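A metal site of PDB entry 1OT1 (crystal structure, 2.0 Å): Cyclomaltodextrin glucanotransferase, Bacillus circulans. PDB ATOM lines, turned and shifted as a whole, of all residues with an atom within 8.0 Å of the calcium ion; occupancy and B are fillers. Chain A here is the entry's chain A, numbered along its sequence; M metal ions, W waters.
The backbone carbonyl oxygen (O) of Gly 189 is in hydrogen-bond range of a ring nitrogen (ND1) of His 233, at 2.7 Å. The backbone NH of Asn 139 is in hydrogen-bond range of the side-chain sulfur of Met 234 (3.5 Å). The backbone carbonyl oxygen (O) of Asn 139 lies within hydrogen-bond range of the backbone NH (N) of Leu 200. ND2 of Asn 139 sits at hydrogen-bond distance from ND1 of His 140, at 3.0 Å. The backbone carbonyl oxygen (O) of Asp 199 lies within hydrogen-bond range of the backbone NH (N) of His 176, at 2.8 Å. N of Asp 199 lies close to OD1 of Asn 193, 3.2 Å away.
Water W3 lies within hydrogen-bond range of O of Asn 139 (2.7 Å) and O of Leu 200 (2.9 Å).
Of the 24 residues printed, 4 come within 4 Å of the calcium ion. Along chain A the residues within 4 Å of the calcium ion span positions 139 to 233.
The backbone carbonyl oxygen (O) of His 233 binds the calcium ion, at 2.4 Å. The calcium ion is bound by the side-chain amide oxygen (OD1) of Asn 139, 2.4 Å away. Water W3 is bound to the calcium ion. The calcium ion is bound by water W2 (2.4 Å). The calcium ion is bound by water W1 (2.5 Å). OD2 of Asp 199 is bound to the calcium ion, 2.5 Å away. O of Ile 190 is bound to the calcium ion (2.5 Å). The side-chain carboxylate (OD1) of Asp 199 is bound to the calcium ion, 2.5 Å away.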
ATOM      1  N   PRO A 138     -21.722 -30.429  -7.472  1.00  0.00           N
ATOM      2  CA  PRO A 138     -22.230 -30.689  -8.819  1.00  0.00           C
ATOM      3  C   PRO A 138     -22.760 -29.474  -9.582  1.00  0.00           C
ATOM      4  O   PRO A 138     -23.405 -29.629 -10.613  1.00  0.00           O
ATOM      5  CB  PRO A 138     -23.321 -31.729  -8.564  1.00  0.00           C
ATOM      6  CG  PRO A 138     -23.897 -31.237  -7.267  1.00  0.00           C
ATOM      7  CD  PRO A 138     -22.675 -30.907  -6.447  1.00  0.00           C
ATOM      8  N   ASN A 139     -22.494 -28.271  -9.084  1.00  0.00           N
ATOM      9  CA  ASN A 139     -22.976 -27.067  -9.747  1.00  0.00           C
ATOM     10  C   ASN A 139     -22.118 -26.685 -10.958  1.00  0.00           C
ATOM     11  O   ASN A 139     -22.608 -26.079 -11.905  1.00  0.00           O
ATOM     12  CB  ASN A 139     -22.967 -25.877  -8.788  1.00  0.00           C
ATOM     13  CG  ASN A 139     -23.346 -24.568  -9.465  1.00  0.00           C
ATOM     14  OD1 ASN A 139     -24.503 -24.372  -9.869  1.00  0.00           O
ATOM     15  ND2 ASN A 139     -22.384 -23.670  -9.616  1.00  0.00           N
ATOM     16  N   HIS A 140     -20.841 -27.062 -10.919  1.00  0.00           N
ATOM     17  CA  HIS A 140     -19.905 -26.661 -11.962  1.00  0.00           C
ATOM     18  C   HIS A 140     -18.721 -27.600 -12.048  1.00  0.00           C
ATOM     19  O   HIS A 140     -18.561 -28.507 -11.219  1.00  0.00           O
ATOM     20  CB  HIS A 140     -19.378 -25.270 -11.629  1.00  0.00           C
ATOM     21  CG  HIS A 140     -18.839 -25.160 -10.245  1.00  0.00           C
ATOM     22  ND1 HIS A 140     -19.593 -24.729  -9.176  1.00  0.00           N
ATOM     23  CD2 HIS A 140     -17.633 -25.509  -9.727  1.00  0.00           C
ATOM     24  CE1 HIS A 140     -18.888 -24.817  -8.071  1.00  0.00           C
ATOM     25  NE2 HIS A 140     -17.692 -25.288  -8.377  1.00  0.00           N
ATOM     26  N   HIS A 176     -23.995 -24.099 -19.111  1.00  0.00           N
ATOM     27  CA  HIS A 176     -24.784 -22.905 -19.362  1.00  0.00           C
ATOM     28  C   HIS A 176     -23.869 -21.863 -20.004  1.00  0.00           C
ATOM     29  O   HIS A 176     -22.693 -21.771 -19.657  1.00  0.00           O
ATOM     30  CB  HIS A 176     -25.358 -22.346 -18.063  1.00  0.00           C
ATOM     31  CG  HIS A 176     -26.532 -23.107 -17.553  1.00  0.00           C
ATOM     32  ND1 HIS A 176     -26.765 -23.311 -16.204  1.00  0.00           N
ATOM     33  CD2 HIS A 176     -27.579 -23.681 -18.199  1.00  0.00           C
ATOM     34  CE1 HIS A 176     -27.891 -23.982 -16.051  1.00  0.00           C
ATOM     35  NE2 HIS A 176     -28.403 -24.219 -17.252  1.00  0.00           N
ATOM     36  N   GLU A 187     -32.936 -16.746  -9.536  1.00  0.00           N
ATOM     37  CA  GLU A 187     -32.868 -17.296 -10.892  1.00  0.00           C
ATOM     38  C   GLU A 187     -31.542 -16.946 -11.556  1.00  0.00           C
ATOM     39  O   GLU A 187     -30.909 -17.787 -12.197  1.00  0.00           O
ATOM     40  CB  GLU A 187     -34.016 -16.773 -11.758  1.00  0.00           C
ATOM     41  CG  GLU A 187     -33.841 -17.060 -13.243  1.00  0.00           C
ATOM     42  CD  GLU A 187     -34.910 -16.434 -14.126  1.00  0.00           C
ATOM     43  OE1 GLU A 187     -35.557 -15.466 -13.677  1.00  0.00           O
ATOM     44  OE2 GLU A 187     -35.093 -16.903 -15.265  1.00  0.00           O
ATOM     45  N   ASN A 188     -31.133 -15.686 -11.413  1.00  0.00           N
ATOM     46  CA  ASN A 188     -29.875 -15.197 -11.996  1.00  0.00           C
ATOM     47  C   ASN A 188     -28.699 -16.013 -11.473  1.00  0.00           C
ATOM     48  O   ASN A 188     -27.805 -16.398 -12.240  1.00  0.00           O
ATOM     49  CB  ASN A 188     -29.696 -13.708 -11.656  1.00  0.00           C
ATOM     50  CG  ASN A 188     -28.450 -13.108 -12.309  1.00  0.00           C
ATOM     51  OD1 ASN A 188     -27.325 -13.393 -11.908  1.00  0.00           O
ATOM     52  ND2 ASN A 188     -28.671 -12.260 -13.305  1.00  0.00           N
ATOM     53  N   GLY A 189     -28.702 -16.291 -10.171  1.00  0.00           N
ATOM     54  CA  GLY A 189     -27.623 -17.048  -9.567  1.00  0.00           C
ATOM     55  C   GLY A 189     -27.623 -18.538  -9.893  1.00  0.00           C
ATOM     56  O   GLY A 189     -26.617 -19.222  -9.722  1.00  0.00           O
ATOM     57  N   ILE A 190     -28.753 -19.041 -10.387  1.00  0.00           N
ATOM     58  CA  ILE A 190     -28.852 -20.455 -10.731  1.00  0.00           C
ATOM     59  C   ILE A 190     -28.427 -20.784 -12.164  1.00  0.00           C
ATOM     60  O   ILE A 190     -27.653 -21.715 -12.389  1.00  0.00           O
ATOM     61  CB  ILE A 190     -30.300 -20.985 -10.532  1.00  0.00           C
ATOM     62  CG1 ILE A 190     -30.646 -21.027  -9.035  1.00  0.00           C
ATOM     63  CG2 ILE A 190     -30.441 -22.380 -11.143  1.00  0.00           C
ATOM     64  CD1 ILE A 190     -32.079 -21.424  -8.755  1.00  0.00           C
ATOM     65  N   TYR A 191     -28.919 -20.005 -13.116  1.00  0.00           N
ATOM     66  CA  TYR A 191     -28.649 -20.290 -14.522  1.00  0.00           C
ATOM     67  C   TYR A 191     -27.501 -19.520 -15.172  1.00  0.00           C
ATOM     68  O   TYR A 191     -27.350 -19.537 -16.406  1.00  0.00           O
ATOM     69  CB  TYR A 191     -29.956 -20.116 -15.307  1.00  0.00           C
ATOM     70  CG  TYR A 191     -31.009 -21.107 -14.870  1.00  0.00           C
ATOM     71  CD1 TYR A 191     -30.953 -22.446 -15.285  1.00  0.00           C
ATOM     72  CD2 TYR A 191     -32.019 -20.742 -13.978  1.00  0.00           C
ATOM     73  CE1 TYR A 191     -31.884 -23.390 -14.815  1.00  0.00           C
ATOM     74  CE2 TYR A 191     -32.942 -21.666 -13.510  1.00  0.00           C
ATOM     75  CZ  TYR A 191     -32.869 -22.987 -13.927  1.00  0.00           C
ATOM     76  OH  TYR A 191     -33.792 -23.908 -13.468  1.00  0.00           O
ATOM     77  N   LYS A 192     -26.693 -18.864 -14.350  1.00  0.00           N
ATOM     78  CA  LYS A 192     -25.506 -18.155 -14.823  1.00  0.00           C
ATOM     79  C   LYS A 192     -24.326 -18.681 -14.007  1.00  0.00           C
ATOM     80  O   LYS A 192     -24.524 -19.273 -12.938  1.00  0.00           O
ATOM     81  CB  LYS A 192     -25.656 -16.642 -14.650  1.00  0.00           C
ATOM     82  CG  LYS A 192     -26.752 -16.031 -15.499  1.00  0.00           C
ATOM     83  CD  LYS A 192     -26.620 -14.517 -15.606  1.00  0.00           C
ATOM     84  CE  LYS A 192     -27.663 -13.941 -16.556  1.00  0.00           C
ATOM     85  NZ  LYS A 192     -27.380 -12.520 -16.909  1.00  0.00           N
ATOM     86  N   ASN A 193     -23.107 -18.474 -14.501  1.00  0.00           N
ATOM     87  CA  ASN A 193     -21.910 -18.987 -13.817  1.00  0.00           C
ATOM     88  C   ASN A 193     -21.545 -18.298 -12.512  1.00  0.00           C
ATOM     89  O   ASN A 193     -21.751 -17.091 -12.346  1.00  0.00           O
ATOM     90  CB  ASN A 193     -20.673 -18.895 -14.722  1.00  0.00           C
ATOM     91  CG  ASN A 193     -20.851 -19.597 -16.048  1.00  0.00           C
ATOM     92  OD1 ASN A 193     -21.648 -20.519 -16.182  1.00  0.00           O
ATOM     93  ND2 ASN A 193     -20.077 -19.170 -17.041  1.00  0.00           N
ATOM     94  N   LEU A 194     -21.003 -19.087 -11.578  1.00  0.00           N
ATOM     95  CA  LEU A 194     -20.461 -18.560 -10.336  1.00  0.00           C
ATOM     96  C   LEU A 194     -19.034 -18.216 -10.732  1.00  0.00           C
ATOM     97  O   LEU A 194     -18.312 -19.095 -11.214  1.00  0.00           O
ATOM     98  CB  LEU A 194     -20.416 -19.630  -9.250  1.00  0.00           C
ATOM     99  CG  LEU A 194     -21.670 -19.951  -8.437  1.00  0.00           C
ATOM    100  CD1 LEU A 194     -21.329 -21.025  -7.406  1.00  0.00           C
ATOM    101  CD2 LEU A 194     -22.173 -18.688  -7.749  1.00  0.00           C
ATOM    102  N   LEU A 197     -16.586 -20.146 -13.270  1.00  0.00           N
ATOM    103  CA  LEU A 197     -16.776 -21.589 -13.231  1.00  0.00           C
ATOM    104  C   LEU A 197     -17.833 -22.061 -14.238  1.00  0.00           C
ATOM    105  O   LEU A 197     -18.955 -21.547 -14.249  1.00  0.00           O
ATOM    106  CB  LEU A 197     -17.170 -22.034 -11.818  1.00  0.00           C
ATOM    107  CG  LEU A 197     -16.200 -21.622 -10.695  1.00  0.00           C
ATOM    108  CD1 LEU A 197     -16.797 -22.014  -9.346  1.00  0.00           C
ATOM    109  CD2 LEU A 197     -14.843 -22.292 -10.898  1.00  0.00           C
ATOM    110  N   ALA A 198     -17.471 -23.040 -15.061  1.00  0.00           N
ATOM    111  CA  ALA A 198     -18.385 -23.588 -16.063  1.00  0.00           C
ATOM    112  C   ALA A 198     -19.607 -24.208 -15.383  1.00  0.00           C
ATOM    113  O   ALA A 198     -19.506 -25.257 -14.740  1.00  0.00           O
ATOM    114  CB  ALA A 198     -17.670 -24.649 -16.908  1.00  0.00           C
ATOM    115  N   ASP A 199     -20.750 -23.549 -15.539  1.00  0.00           N
ATOM    116  CA  ASP A 199     -21.981 -23.990 -14.903  1.00  0.00           C
ATOM    117  C   ASP A 199     -22.580 -25.214 -15.594  1.00  0.00           C
ATOM    118  O   ASP A 199     -22.888 -25.175 -16.788  1.00  0.00           O
ATOM    119  CB  ASP A 199     -23.003 -22.842 -14.915  1.00  0.00           C
ATOM    120  CG  ASP A 199     -23.971 -22.913 -13.762  1.00  0.00           C
ATOM    121  OD1 ASP A 199     -23.502 -22.918 -12.598  1.00  0.00           O
ATOM    122  OD2 ASP A 199     -25.190 -22.974 -14.008  1.00  0.00           O
ATOM    123  N   LEU A 200     -22.746 -26.293 -14.839  1.00  0.00           N
ATOM    124  CA  LEU A 200     -23.314 -27.513 -15.396  1.00  0.00           C
ATOM    125  C   LEU A 200     -24.814 -27.351 -15.668  1.00  0.00           C
ATOM    126  O   LEU A 200     -25.536 -26.725 -14.890  1.00  0.00           O
ATOM    127  CB  LEU A 200     -23.073 -28.695 -14.459  1.00  0.00           C
ATOM    128  CG  LEU A 200     -21.650 -29.259 -14.477  1.00  0.00           C
ATOM    129  CD1 LEU A 200     -21.447 -30.240 -13.326  1.00  0.00           C
ATOM    130  CD2 LEU A 200     -21.388 -29.949 -15.823  1.00  0.00           C
ATOM    131  N   ASN A 201     -25.265 -27.915 -16.782  1.00  0.00           N
ATOM    132  CA  ASN A 201     -26.661 -27.853 -17.180  1.00  0.00           C
ATOM    133  C   ASN A 201     -27.356 -29.149 -16.778  1.00  0.00           C
ATOM    134  O   ASN A 201     -27.279 -30.147 -17.498  1.00  0.00           O
ATOM    135  CB  ASN A 201     -26.765 -27.646 -18.693  1.00  0.00           C
ATOM    136  CG  ASN A 201     -28.185 -27.745 -19.204  1.00  0.00           C
ATOM    137  OD1 ASN A 201     -29.142 -27.596 -18.443  1.00  0.00           O
ATOM    138  ND2 ASN A 201     -28.333 -27.977 -20.513  1.00  0.00           N
ATOM    139  N   HIS A 202     -28.028 -29.137 -15.640  1.00  0.00           N
ATOM    140  CA  HIS A 202     -28.680 -30.337 -15.145  1.00  0.00           C
ATOM    141  C   HIS A 202     -29.903 -30.758 -15.933  1.00  0.00           C
ATOM    142  O   HIS A 202     -30.480 -31.819 -15.688  1.00  0.00           O
ATOM    143  CB  HIS A 202     -29.026 -30.170 -13.661  1.00  0.00           C
ATOM    144  CG  HIS A 202     -27.832 -29.828 -12.819  1.00  0.00           C
ATOM    145  ND1 HIS A 202     -27.434 -28.534 -12.581  1.00  0.00           N
ATOM    146  CD2 HIS A 202     -26.904 -30.621 -12.217  1.00  0.00           C
ATOM    147  CE1 HIS A 202     -26.318 -28.532 -11.868  1.00  0.00           C
ATOM    148  NE2 HIS A 202     -25.975 -29.787 -11.637  1.00  0.00           N
ATOM    149  N   ALA A 230     -22.957 -24.914  -2.835  1.00  0.00           N
ATOM    150  CA  ALA A 230     -23.654 -23.962  -3.702  1.00  0.00           C
ATOM    151  C   ALA A 230     -25.071 -24.375  -4.109  1.00  0.00           C
ATOM    152  O   ALA A 230     -25.429 -24.268  -5.286  1.00  0.00           O
ATOM    153  CB  ALA A 230     -22.804 -23.721  -4.951  1.00  0.00           C
ATOM    154  N   VAL A 231     -25.874 -24.823  -3.149  1.00  0.00           N
ATOM    155  CA  VAL A 231     -27.232 -25.274  -3.486  1.00  0.00           C
ATOM    156  C   VAL A 231     -28.182 -24.149  -3.879  1.00  0.00           C
ATOM    157  O   VAL A 231     -29.207 -24.398  -4.505  1.00  0.00           O
ATOM    158  CB  VAL A 231     -27.868 -26.076  -2.326  1.00  0.00           C
ATOM    159  CG1 VAL A 231     -27.021 -27.316  -2.040  1.00  0.00           C
ATOM    160  CG2 VAL A 231     -27.990 -25.210  -1.092  1.00  0.00           C
ATOM    161  N   LYS A 232     -27.848 -22.910  -3.530  1.00  0.00           N
ATOM    162  CA  LYS A 232     -28.705 -21.794  -3.925  1.00  0.00           C
ATOM    163  C   LYS A 232     -28.480 -21.497  -5.414  1.00  0.00           C
ATOM    164  O   LYS A 232     -29.195 -20.703  -6.007  1.00  0.00           O
ATOM    165  CB  LYS A 232     -28.391 -20.529  -3.110  1.00  0.00           C
ATOM    166  CG  LYS A 232     -29.352 -19.373  -3.399  1.00  0.00           C
ATOM    167  CD  LYS A 232     -29.001 -18.097  -2.618  1.00  0.00           C
ATOM    168  CE  LYS A 232     -30.012 -16.990  -2.909  1.00  0.00           C
ATOM    169  NZ  LYS A 232     -29.646 -15.680  -2.285  1.00  0.00           N
ATOM    170  N   HIS A 233     -27.493 -22.178  -6.003  1.00  0.00           N
ATOM    171  CA  HIS A 233     -27.139 -21.932  -7.395  1.00  0.00           C
ATOM    172  C   HIS A 233     -27.432 -23.056  -8.382  1.00  0.00           C
ATOM    173  O   HIS A 233     -26.981 -23.032  -9.527  1.00  0.00           O
ATOM    174  CB  HIS A 233     -25.666 -21.534  -7.455  1.00  0.00           C
ATOM    175  CG  HIS A 233     -25.367 -20.283  -6.680  1.00  0.00           C
ATOM    176  ND1 HIS A 233     -25.608 -19.024  -7.184  1.00  0.00           N
ATOM    177  CD2 HIS A 233     -24.933 -20.115  -5.407  1.00  0.00           C
ATOM    178  CE1 HIS A 233     -25.343 -18.129  -6.248  1.00  0.00           C
ATOM    179  NE2 HIS A 233     -24.937 -18.757  -5.171  1.00  0.00           N
ATOM    180  N   MET A 234     -28.210 -24.048  -7.928  1.00  0.00           N
ATOM    181  CA  MET A 234     -28.637 -25.153  -8.788  1.00  0.00           C
ATOM    182  C   MET A 234     -30.158 -25.184  -8.724  1.00  0.00           C
ATOM    183  O   MET A 234     -30.754 -24.730  -7.742  1.00  0.00           O
ATOM    184  CB  MET A 234     -28.046 -26.473  -8.299  1.00  0.00           C
ATOM    185  CG  MET A 234     -26.523 -26.558  -8.413  1.00  0.00           C
ATOM    186  SD  MET A 234     -25.843 -28.163  -7.914  1.00  0.00           S
ATOM    187  CE  MET A 234     -25.825 -27.950  -6.129  1.00  0.00           C
ATOM    188  N   PRO A 235     -30.819 -25.710  -9.779  1.00  0.00           N
ATOM    189  CA  PRO A 235     -32.284 -25.763  -9.768  1.00  0.00           C
ATOM    190  C   PRO A 235     -32.769 -26.556  -8.564  1.00  0.00           C
ATOM    191  O   PRO A 235     -32.328 -27.685  -8.339  1.00  0.00           O
ATOM    192  CB  PRO A 235     -32.617 -26.452 -11.101  1.00  0.00           C
ATOM    193  CG  PRO A 235     -31.454 -26.062 -11.977  1.00  0.00           C
ATOM    194  CD  PRO A 235     -30.286 -26.232 -11.050  1.00  0.00           C
HETATM  195 CA    CA M   1     -25.809 -23.260 -11.567  1.00  0.00          CA
HETATM  196  O   HOH W   1     -27.852 -24.426 -12.344  1.00  0.00           O
HETATM  197  O   HOH W   2     -24.916 -21.102 -10.863  1.00  0.00           O
HETATM  198  O   HOH W   3     -25.196 -25.489 -12.287  1.00  0.00           O
